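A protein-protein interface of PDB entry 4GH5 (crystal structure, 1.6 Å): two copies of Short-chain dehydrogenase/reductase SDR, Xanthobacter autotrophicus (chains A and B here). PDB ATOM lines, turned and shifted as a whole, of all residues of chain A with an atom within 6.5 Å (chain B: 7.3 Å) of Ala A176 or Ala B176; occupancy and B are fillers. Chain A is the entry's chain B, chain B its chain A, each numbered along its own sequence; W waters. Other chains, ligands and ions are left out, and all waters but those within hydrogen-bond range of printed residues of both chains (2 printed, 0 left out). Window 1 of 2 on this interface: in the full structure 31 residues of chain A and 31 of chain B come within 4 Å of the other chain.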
ATOM      1  N   MET A 126     -22.719  13.712  22.063  1.00  0.00           N
ATOM      2  CA  MET A 126     -21.424  13.383  22.663  1.00  0.00           C
ATOM      3  C   MET A 126     -20.530  14.624  22.804  1.00  0.00           C
ATOM      4  O   MET A 126     -19.843  14.797  23.813  1.00  0.00           O
ATOM      5  CB  MET A 126     -20.701  12.308  21.849  1.00  0.00           C
ATOM      6  CG  MET A 126     -21.407  10.960  21.799  1.00  0.00           C
ATOM      7  SD  MET A 126     -21.477  10.140  23.413  1.00  0.00           S
ATOM      8  CE  MET A 126     -19.777   9.934  23.733  1.00  0.00           C
ATOM      9  N   VAL A 130     -19.707  15.389  26.517  1.00  0.00           N
ATOM     10  CA  VAL A 130     -18.396  14.859  26.856  1.00  0.00           C
ATOM     11  C   VAL A 130     -17.260  15.799  26.458  1.00  0.00           C
ATOM     12  O   VAL A 130     -16.429  16.151  27.288  1.00  0.00           O
ATOM     13  CB  VAL A 130     -18.161  13.462  26.252  1.00  0.00           C
ATOM     14  CG1 VAL A 130     -16.851  12.873  26.792  1.00  0.00           C
ATOM     15  CG2 VAL A 130     -19.337  12.537  26.573  1.00  0.00           C
ATOM     16  N   GLY A 160     -26.842   8.304  33.000  1.00  0.00           N
ATOM     17  CA  GLY A 160     -25.450   7.907  32.914  1.00  0.00           C
ATOM     18  C   GLY A 160     -25.117   6.717  33.789  1.00  0.00           C
ATOM     19  O   GLY A 160     -24.009   6.179  33.717  1.00  0.00           O
ATOM     20  N   CYS A 171     -27.241   8.380  26.831  1.00  0.00           N
ATOM     21  CA  CYS A 171     -26.813   7.442  27.861  1.00  0.00           C
ATOM     22  C   CYS A 171     -25.331   7.143  27.737  1.00  0.00           C
ATOM     23  O   CYS A 171     -24.658   6.914  28.749  1.00  0.00           O
ATOM     24  CB  CYS A 171     -27.607   6.146  27.770  1.00  0.00           C
ATOM     25  SG  CYS A 171     -29.292   6.329  28.428  1.00  0.00           S
ATOM     26  N   ALA A 172     -24.839   7.113  26.493  1.00  0.00           N
ATOM     27  CA  ALA A 172     -23.414   6.937  26.247  1.00  0.00           C
ATOM     28  C   ALA A 172     -22.662   8.152  26.787  1.00  0.00           C
ATOM     29  O   ALA A 172     -21.658   8.001  27.485  1.00  0.00           O
ATOM     30  CB  ALA A 172     -23.135   6.761  24.746  1.00  0.00           C
ATOM     31  N   ALA A 173     -23.167   9.347  26.473  1.00  0.00           N
ATOM     32  CA  ALA A 173     -22.516  10.603  26.868  1.00  0.00           C
ATOM     33  C   ALA A 173     -22.463  10.762  28.386  1.00  0.00           C
ATOM     34  O   ALA A 173     -21.409  11.071  28.959  1.00  0.00           O
ATOM     35  CB  ALA A 173     -23.212  11.794  26.215  1.00  0.00           C
ATOM     36  N   LYS A 174     -23.587  10.505  29.044  1.00  0.00           N
ATOM     37  CA  LYS A 174     -23.617  10.652  30.490  1.00  0.00           C
ATOM     38  C   LYS A 174     -22.827   9.528  31.172  1.00  0.00           C
ATOM     39  O   LYS A 174     -22.187   9.741  32.202  1.00  0.00           O
ATOM     40  CB  LYS A 174     -25.055  10.757  31.010  1.00  0.00           C
ATOM     41  CG  LYS A 174     -25.793  12.042  30.538  1.00  0.00           C
ATOM     42  CD  LYS A 174     -24.935  13.311  30.802  1.00  0.00           C
ATOM     43  CE  LYS A 174     -25.790  14.558  30.790  1.00  0.00           C
ATOM     44  NZ  LYS A 174     -24.973  15.795  31.019  1.00  0.00           N
ATOM     45  N   GLY A 175     -22.840   8.338  30.579  1.00  0.00           N
ATOM     46  CA  GLY A 175     -21.974   7.268  31.049  1.00  0.00           C
ATOM     47  C   GLY A 175     -20.504   7.669  30.968  1.00  0.00           C
ATOM     48  O   GLY A 175     -19.729   7.423  31.885  1.00  0.00           O
ATOM     49  N   ALA A 176     -20.119   8.309  29.866  1.00  0.00           N
ATOM     50  CA  ALA A 176     -18.751   8.812  29.735  1.00  0.00           C
ATOM     51  C   ALA A 176     -18.402   9.811  30.840  1.00  0.00           C
ATOM     52  O   ALA A 176     -17.318   9.752  31.431  1.00  0.00           O
ATOM     53  CB  ALA A 176     -18.541   9.455  28.358  1.00  0.00           C
ATOM     54  N   ILE A 177     -19.315  10.737  31.104  1.00  0.00           N
ATOM     55  CA  ILE A 177     -19.064  11.775  32.100  1.00  0.00           C
ATOM     56  C   ILE A 177     -18.876  11.167  33.493  1.00  0.00           C
ATOM     57  O   ILE A 177     -17.973  11.572  34.227  1.00  0.00           O
ATOM     58  CB  ILE A 177     -20.169  12.843  32.086  1.00  0.00           C
ATOM     59  CG1 ILE A 177     -20.063  13.662  30.793  1.00  0.00           C
ATOM     60  CG2 ILE A 177     -20.067  13.748  33.317  1.00  0.00           C
ATOM     61  CD1 ILE A 177     -21.259  14.583  30.563  1.00  0.00           C
ATOM     62  N   VAL A 178     -19.698  10.175  33.837  1.00  0.00           N
ATOM     63  CA  VAL A 178     -19.580   9.535  35.138  1.00  0.00           C
ATOM     64  C   VAL A 178     -18.189   8.941  35.316  1.00  0.00           C
ATOM     65  O   VAL A 178     -17.537   9.182  36.327  1.00  0.00           O
ATOM     66  CB  VAL A 178     -20.654   8.450  35.331  1.00  0.00           C
ATOM     67  CG1 VAL A 178     -20.352   7.597  36.561  1.00  0.00           C
ATOM     68  CG2 VAL A 178     -22.037   9.109  35.476  1.00  0.00           C
ATOM     69  N   ASN A 179     -17.698   8.200  34.326  1.00  0.00           N
ATOM     70  CA  ASN A 179     -16.382   7.611  34.543  1.00  0.00           C
ATOM     71  C   ASN A 179     -15.221   8.566  34.305  1.00  0.00           C
ATOM     72  O   ASN A 179     -14.171   8.430  34.938  1.00  0.00           O
ATOM     73  CB  ASN A 179     -16.185   6.284  33.800  1.00  0.00           C
ATOM     74  CG  ASN A 179     -15.080   5.458  34.421  1.00  0.00           C
ATOM     75  OD1 ASN A 179     -15.154   5.127  35.601  1.00  0.00           O
ATOM     76  ND2 ASN A 179     -14.045   5.133  33.651  1.00  0.00           N
ATOM     77  N   LEU A 180     -15.404   9.531  33.401  1.00  0.00           N
ATOM     78  CA  LEU A 180     -14.403  10.588  33.223  1.00  0.00           C
ATOM     79  C   LEU A 180     -14.178  11.318  34.535  1.00  0.00           C
ATOM     80  O   LEU A 180     -13.052  11.692  34.875  1.00  0.00           O
ATOM     81  CB  LEU A 180     -14.851  11.592  32.161  1.00  0.00           C
ATOM     82  CG  LEU A 180     -13.961  12.817  31.942  1.00  0.00           C
ATOM     83  CD1 LEU A 180     -12.517  12.387  31.610  1.00  0.00           C
ATOM     84  CD2 LEU A 180     -14.554  13.682  30.837  1.00  0.00           C
ATOM     85  N   THR A 181     -15.264  11.506  35.279  1.00  0.00           N
ATOM     86  CA  THR A 181     -15.182  12.131  36.591  1.00  0.00           C
ATOM     87  C   THR A 181     -14.258  11.353  37.535  1.00  0.00           C
ATOM     88  O   THR A 181     -13.412  11.943  38.219  1.00  0.00           O
ATOM     89  CB  THR A 181     -16.577  12.270  37.224  1.00  0.00           C
ATOM     90  OG1 THR A 181     -17.378  13.125  36.403  1.00  0.00           O
ATOM     91  CG2 THR A 181     -16.468  12.857  38.620  1.00  0.00           C
ATOM     92  N   TRP B 122      -8.147  12.623  21.504  1.00  0.00           N
ATOM     93  CA  TRP B 122      -9.353  12.403  22.308  1.00  0.00           C
ATOM     94  C   TRP B 122     -10.479  11.936  21.391  1.00  0.00           C
ATOM     95  O   TRP B 122     -11.113  10.897  21.633  1.00  0.00           O
ATOM     96  CB  TRP B 122      -9.765  13.705  23.018  1.00  0.00           C
ATOM     97  CG  TRP B 122     -11.008  13.580  23.856  1.00  0.00           C
ATOM     98  CD1 TRP B 122     -12.297  13.467  23.413  1.00  0.00           C
ATOM     99  CD2 TRP B 122     -11.073  13.554  25.284  1.00  0.00           C
ATOM    100  NE1 TRP B 122     -13.158  13.362  24.478  1.00  0.00           N
ATOM    101  CE2 TRP B 122     -12.435  13.424  25.639  1.00  0.00           C
ATOM    102  CE3 TRP B 122     -10.113  13.648  26.299  1.00  0.00           C
ATOM    103  CZ2 TRP B 122     -12.858  13.359  26.971  1.00  0.00           C
ATOM    104  CZ3 TRP B 122     -10.535  13.596  27.615  1.00  0.00           C
ATOM    105  CH2 TRP B 122     -11.894  13.449  27.939  1.00  0.00           C
ATOM    106  N   MET B 126     -12.470   8.260  21.337  1.00  0.00           N
ATOM    107  CA  MET B 126     -13.912   8.181  21.491  1.00  0.00           C
ATOM    108  C   MET B 126     -14.548   7.552  20.257  1.00  0.00           C
ATOM    109  O   MET B 126     -15.511   6.792  20.367  1.00  0.00           O
ATOM    110  CB  MET B 126     -14.503   9.571  21.740  1.00  0.00           C
ATOM    111  CG  MET B 126     -14.094  10.190  23.066  1.00  0.00           C
ATOM    112  SD  MET B 126     -14.757   9.307  24.493  1.00  0.00           S
ATOM    113  CE  MET B 126     -16.475   9.543  24.265  1.00  0.00           C
ATOM    114  N   ASN B 129     -13.803   3.491  19.890  1.00  0.00           N
ATOM    115  CA  ASN B 129     -14.513   2.797  20.957  1.00  0.00           C
ATOM    116  C   ASN B 129     -16.031   3.011  20.925  1.00  0.00           C
ATOM    117  O   ASN B 129     -16.800   2.056  20.774  1.00  0.00           O
ATOM    118  CB  ASN B 129     -13.957   3.221  22.324  1.00  0.00           C
ATOM    119  CG  ASN B 129     -12.571   2.677  22.579  1.00  0.00           C
ATOM    120  OD1 ASN B 129     -12.411   1.499  22.902  1.00  0.00           O
ATOM    121  ND2 ASN B 129     -11.553   3.530  22.436  1.00  0.00           N
ATOM    122  N   VAL B 130     -16.454   4.260  21.085  1.00  0.00           N
ATOM    123  CA  VAL B 130     -17.877   4.540  21.249  1.00  0.00           C
ATOM    124  C   VAL B 130     -18.617   4.559  19.915  1.00  0.00           C
ATOM    125  O   VAL B 130     -19.584   3.828  19.723  1.00  0.00           O
ATOM    126  CB  VAL B 130     -18.130   5.865  21.998  1.00  0.00           C
ATOM    127  CG1 VAL B 130     -19.612   5.988  22.321  1.00  0.00           C
ATOM    128  CG2 VAL B 130     -17.304   5.914  23.295  1.00  0.00           C
ATOM    129  N   GLY B 160     -13.366   1.410  32.331  1.00  0.00           N
ATOM    130  CA  GLY B 160     -14.695   1.947  32.116  1.00  0.00           C
ATOM    131  C   GLY B 160     -15.520   2.009  33.384  1.00  0.00           C
ATOM    132  O   GLY B 160     -16.602   2.586  33.387  1.00  0.00           O
ATOM    133  N   ALA B 168      -7.624   9.940  30.279  1.00  0.00           N
ATOM    134  CA  ALA B 168      -8.922  10.603  30.300  1.00  0.00           C
ATOM    135  C   ALA B 168      -9.876  10.177  29.172  1.00  0.00           C
ATOM    136  O   ALA B 168     -11.010   9.757  29.438  1.00  0.00           O
ATOM    137  CB  ALA B 168      -8.740  12.132  30.323  1.00  0.00           C
ATOM    138  N   ALA B 169      -9.434  10.274  27.915  1.00  0.00           N
ATOM    139  CA  ALA B 169     -10.322   9.917  26.813  1.00  0.00           C
ATOM    140  C   ALA B 169     -10.744   8.444  26.856  1.00  0.00           C
ATOM    141  O   ALA B 169     -11.905   8.111  26.594  1.00  0.00           O
ATOM    142  CB  ALA B 169      -9.676  10.258  25.473  1.00  0.00           C
ATOM    143  N   TYR B 170      -9.799   7.577  27.197  1.00  0.00           N
ATOM    144  CA  TYR B 170     -10.043   6.141  27.217  1.00  0.00           C
ATOM    145  C   TYR B 170     -11.034   5.784  28.326  1.00  0.00           C
ATOM    146  O   TYR B 170     -11.936   4.974  28.120  1.00  0.00           O
ATOM    147  CB  TYR B 170      -8.719   5.394  27.386  1.00  0.00           C
ATOM    148  CG  TYR B 170      -8.839   3.893  27.257  1.00  0.00           C
ATOM    149  CD1 TYR B 170      -9.128   3.295  26.030  1.00  0.00           C
ATOM    150  CD2 TYR B 170      -8.671   3.075  28.366  1.00  0.00           C
ATOM    151  CE1 TYR B 170      -9.238   1.913  25.914  1.00  0.00           C
ATOM    152  CE2 TYR B 170      -8.775   1.710  28.263  1.00  0.00           C
ATOM    153  CZ  TYR B 170      -9.053   1.132  27.047  1.00  0.00           C
ATOM    154  OH  TYR B 170      -9.141  -0.233  26.973  1.00  0.00           O
ATOM    155  N   CYS B 171     -10.889   6.410  29.488  1.00  0.00           N
ATOM    156  CA  CYS B 171     -11.810   6.131  30.588  1.00  0.00           C
ATOM    157  C   CYS B 171     -13.192   6.685  30.256  1.00  0.00           C
ATOM    158  O   CYS B 171     -14.211   6.103  30.631  1.00  0.00           O
ATOM    159  CB  CYS B 171     -11.296   6.730  31.896  1.00  0.00           C
ATOM    160  SG  CYS B 171      -9.925   5.793  32.612  1.00  0.00           S
ATOM    161  N   ALA B 172     -13.234   7.815  29.554  1.00  0.00           N
ATOM    162  CA  ALA B 172     -14.509   8.343  29.082  1.00  0.00           C
ATOM    163  C   ALA B 172     -15.154   7.388  28.088  1.00  0.00           C
ATOM    164  O   ALA B 172     -16.343   7.080  28.191  1.00  0.00           O
ATOM    165  CB  ALA B 172     -14.324   9.716  28.440  1.00  0.00           C
ATOM    166  N   ALA B 173     -14.371   6.914  27.125  1.00  0.00           N
ATOM    167  CA  ALA B 173     -14.897   6.023  26.088  1.00  0.00           C
ATOM    168  C   ALA B 173     -15.415   4.715  26.679  1.00  0.00           C
ATOM    169  O   ALA B 173     -16.511   4.267  26.350  1.00  0.00           O
ATOM    170  CB  ALA B 173     -13.829   5.753  25.040  1.00  0.00           C
ATOM    171  N   LYS B 174     -14.635   4.105  27.554  1.00  0.00           N
ATOM    172  CA  LYS B 174     -15.052   2.824  28.116  1.00  0.00           C
ATOM    173  C   LYS B 174     -16.221   3.016  29.092  1.00  0.00           C
ATOM    174  O   LYS B 174     -17.082   2.152  29.204  1.00  0.00           O
ATOM    175  CB  LYS B 174     -13.870   2.095  28.750  1.00  0.00           C
ATOM    176  CG  LYS B 174     -12.806   1.627  27.730  1.00  0.00           C
ATOM    177  CD  LYS B 174     -13.456   0.844  26.573  1.00  0.00           C
ATOM    178  CE  LYS B 174     -12.429   0.032  25.780  1.00  0.00           C
ATOM    179  NZ  LYS B 174     -13.035  -0.634  24.569  1.00  0.00           N
ATOM    180  N   GLY B 175     -16.269   4.167  29.759  1.00  0.00           N
ATOM    181  CA  GLY B 175     -17.421   4.517  30.577  1.00  0.00           C
ATOM    182  C   GLY B 175     -18.677   4.637  29.719  1.00  0.00           C
ATOM    183  O   GLY B 175     -19.759   4.181  30.099  1.00  0.00           O
ATOM    184  N   ALA B 176     -18.538   5.261  28.556  1.00  0.00           N
ATOM    185  CA  ALA B 176     -19.656   5.372  27.623  1.00  0.00           C
ATOM    186  C   ALA B 176     -20.152   3.996  27.192  1.00  0.00           C
ATOM    187  O   ALA B 176     -21.368   3.733  27.171  1.00  0.00           O
ATOM    188  CB  ALA B 176     -19.238   6.186  26.401  1.00  0.00           C
ATOM    189  N   ILE B 177     -19.217   3.109  26.874  1.00  0.00           N
ATOM    190  CA  ILE B 177     -19.590   1.773  26.424  1.00  0.00           C
ATOM    191  C   ILE B 177     -20.332   1.006  27.514  1.00  0.00           C
ATOM    192  O   ILE B 177     -21.340   0.342  27.237  1.00  0.00           O
ATOM    193  CB  ILE B 177     -18.369   0.991  25.929  1.00  0.00           C
ATOM    194  CG1 ILE B 177     -17.915   1.561  24.585  1.00  0.00           C
ATOM    195  CG2 ILE B 177     -18.709  -0.490  25.777  1.00  0.00           C
ATOM    196  CD1 ILE B 177     -16.508   1.109  24.185  1.00  0.00           C
ATOM    197  N   VAL B 178     -19.854   1.113  28.746  1.00  0.00           N
ATOM    198  CA  VAL B 178     -20.535   0.451  29.862  1.00  0.00           C
ATOM    199  C   VAL B 178     -22.010   0.850  29.974  1.00  0.00           C
ATOM    200  O   VAL B 178     -22.889  -0.014  30.048  1.00  0.00           O
ATOM    201  CB  VAL B 178     -19.792   0.673  31.194  1.00  0.00           C
ATOM    202  CG1 VAL B 178     -20.649   0.181  32.381  1.00  0.00           C
ATOM    203  CG2 VAL B 178     -18.484  -0.085  31.162  1.00  0.00           C
ATOM    204  N   ASN B 179     -22.300   2.147  29.963  1.00  0.00           N
ATOM    205  CA  ASN B 179     -23.700   2.534  30.080  1.00  0.00           C
ATOM    206  C   ASN B 179     -24.492   2.412  28.787  1.00  0.00           C
ATOM    207  O   ASN B 179     -25.688   2.149  28.829  1.00  0.00           O
ATOM    208  CB  ASN B 179     -23.881   3.920  30.673  1.00  0.00           C
ATOM    209  CG  ASN B 179     -25.239   4.073  31.324  1.00  0.00           C
ATOM    210  OD1 ASN B 179     -25.630   3.237  32.155  1.00  0.00           O
ATOM    211  ND2 ASN B 179     -25.984   5.093  30.922  1.00  0.00           N
ATOM    212  N   LEU B 180     -23.837   2.603  27.644  1.00  0.00           N
ATOM    213  CA  LEU B 180     -24.498   2.351  26.362  1.00  0.00           C
ATOM    214  C   LEU B 180     -25.001   0.915  26.290  1.00  0.00           C
ATOM    215  O   LEU B 180     -26.073   0.641  25.734  1.00  0.00           O
ATOM    216  CB  LEU B 180     -23.554   2.633  25.191  1.00  0.00           C
ATOM    217  CG  LEU B 180     -24.066   2.257  23.793  1.00  0.00           C
ATOM    218  CD1 LEU B 180     -25.369   2.984  23.454  1.00  0.00           C
ATOM    219  CD2 LEU B 180     -22.996   2.602  22.760  1.00  0.00           C
ATOM    220  N   THR B 181     -24.229  -0.003  26.865  1.00  0.00           N
ATOM    221  CA  THR B 181     -24.617  -1.402  26.913  1.00  0.00           C
ATOM    222  C   THR B 181     -25.925  -1.571  27.675  1.00  0.00           C
ATOM    223  O   THR B 181     -26.816  -2.289  27.223  1.00  0.00           O
ATOM    224  CB  THR B 181     -23.521  -2.243  27.572  1.00  0.00           C
ATOM    225  OG1 THR B 181     -22.346  -2.188  26.754  1.00  0.00           O
ATOM    226  CG2 THR B 181     -23.975  -3.693  27.741  1.00  0.00           C
ATOM    227  N   ARG B 182     -26.038  -0.890  28.815  1.00  0.00           N
ATOM    228  CA  ARG B 182     -27.271  -0.917  29.594  1.00  0.00           C
ATOM    229  C   ARG B 182     -28.430  -0.369  28.762  1.00  0.00           C
ATOM    230  O   ARG B 182     -29.529  -0.934  28.740  1.00  0.00           O
ATOM    231  CB  ARG B 182     -27.120  -0.111  30.891  1.00  0.00           C
ATOM    232  CG  ARG B 182     -26.082  -0.696  31.856  1.00  0.00           C
ATOM    233  CD  ARG B 182     -26.063   0.064  33.190  1.00  0.00           C
ATOM    234  NE  ARG B 182     -24.936  -0.341  34.028  1.00  0.00           N
ATOM    235  CZ  ARG B 182     -23.876   0.412  34.306  1.00  0.00           C
ATOM    236  NH1 ARG B 182     -23.765   1.655  33.819  1.00  0.00           N
ATOM    237  NH2 ARG B 182     -22.913  -0.082  35.079  1.00  0.00           N
HETATM  238  O   HOH W   1     -20.164   4.847  32.783  1.00  0.00           O
HETATM  239  O   HOH W   2     -22.293   4.217  34.502  1.00  0.00           O
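ND2 of Asn A179 sits at hydrogen-bond distance from O of Cys B171 (3.2 Å).
The backbone carbonyl oxygen (O) of Cys A171 lies within hydrogen-bond range of the side-chain amide nitrogen (ND2) of Asn B179 (3.1 Å).
SD of Met B126 is in hydrogen-bond range of N of Ala B173 (3.6 Å).
OD1 of Asn B179 sits at hydrogen-bond distance from NH1 of Arg B182 (3.0 Å).
SD of Met A126 lies within hydrogen-bond range of N of Ala A173 (3.6 Å).
Among the printed residues, merely in contact across the chains: Met A126 with Met B126 (3.4 Å), Gly A160 with Asn B179 (3.4 Å), Ala A172 with Ala B176 (3.2 Å), Gly A175 with Gly B175 (3.7 Å), Gly A175 with Ala B176 (3.9 Å), Gly A175 with Asn B179 (3.9 Å), Ala A176 with Ala B172 (3.2 Å), Ala A176 with Gly B175 (3.9 Å), Ala A176 with Ala B176 (3.7 Å), Asn A179 with Gly B160 (3.4 Å), Asn A179 with Gly B175 (3.9 Å), Leu A180 with Trp B122 (3.9 Å) and Leu A180 with Ala B168 (3.7 Å).
Of the printed residues of chain B, Ala A172 touches Ala B176 (3.2 Å).
Of the printed residues of chain A, Met B126 touches Met A126 (3.4 Å).
Of the printed residues of chain A, Cys B171 touches Asn A179.
Ala B176 touches just these residues of chain A: Ala A172, Gly A175 and Ala A176.
The nearest residue of chain B that does not touch Ala A176 is Met B126 (4.6 Å).
The nearest residue of chain A that does not touch Ala B176 is Met A126 (4.6 Å).
The nearest printed residue of chain B that does not touch Gly A160 is Arg B182 (4.5 Å).
Hydrophobic or aromatic side chains of chain A within 4 Å of the printed part of chain B: Met A126, Ala A176 and Leu A180.
Printed residues of chain B that touch a printed residue of chain A: Trp B122, Met B126, Gly B160, Ala B168, Cys B171, Ala B172, Gly B175, Ala B176 and Asn B179.
Hydrophobic or aromatic side chains of chain B that line the printed part of chain A: Trp B122, Met B126, Ala B168 and Ala B176.
Met A126 touches its own counterpart, Met B126.
Cys A171 touches Asn B179, and with the chains exchanged Asn A179 touches Cys B171.
Gly A175 touches its own counterpart, Gly B175.
Gly A175 touches Ala B176, and with the chains exchanged Ala A176 touches Gly B175.
Of the 15 pairs that touch across the chains among the printed residues, 13 have their exchanged pair printed and touching as well.
Water W2 bridges O of Gly A160 and NH1 of Arg B182.
Water W1 lies within hydrogen-bond range of O of Gly A175 (2.8 Å) and O of Gly B175 (2.8 Å).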
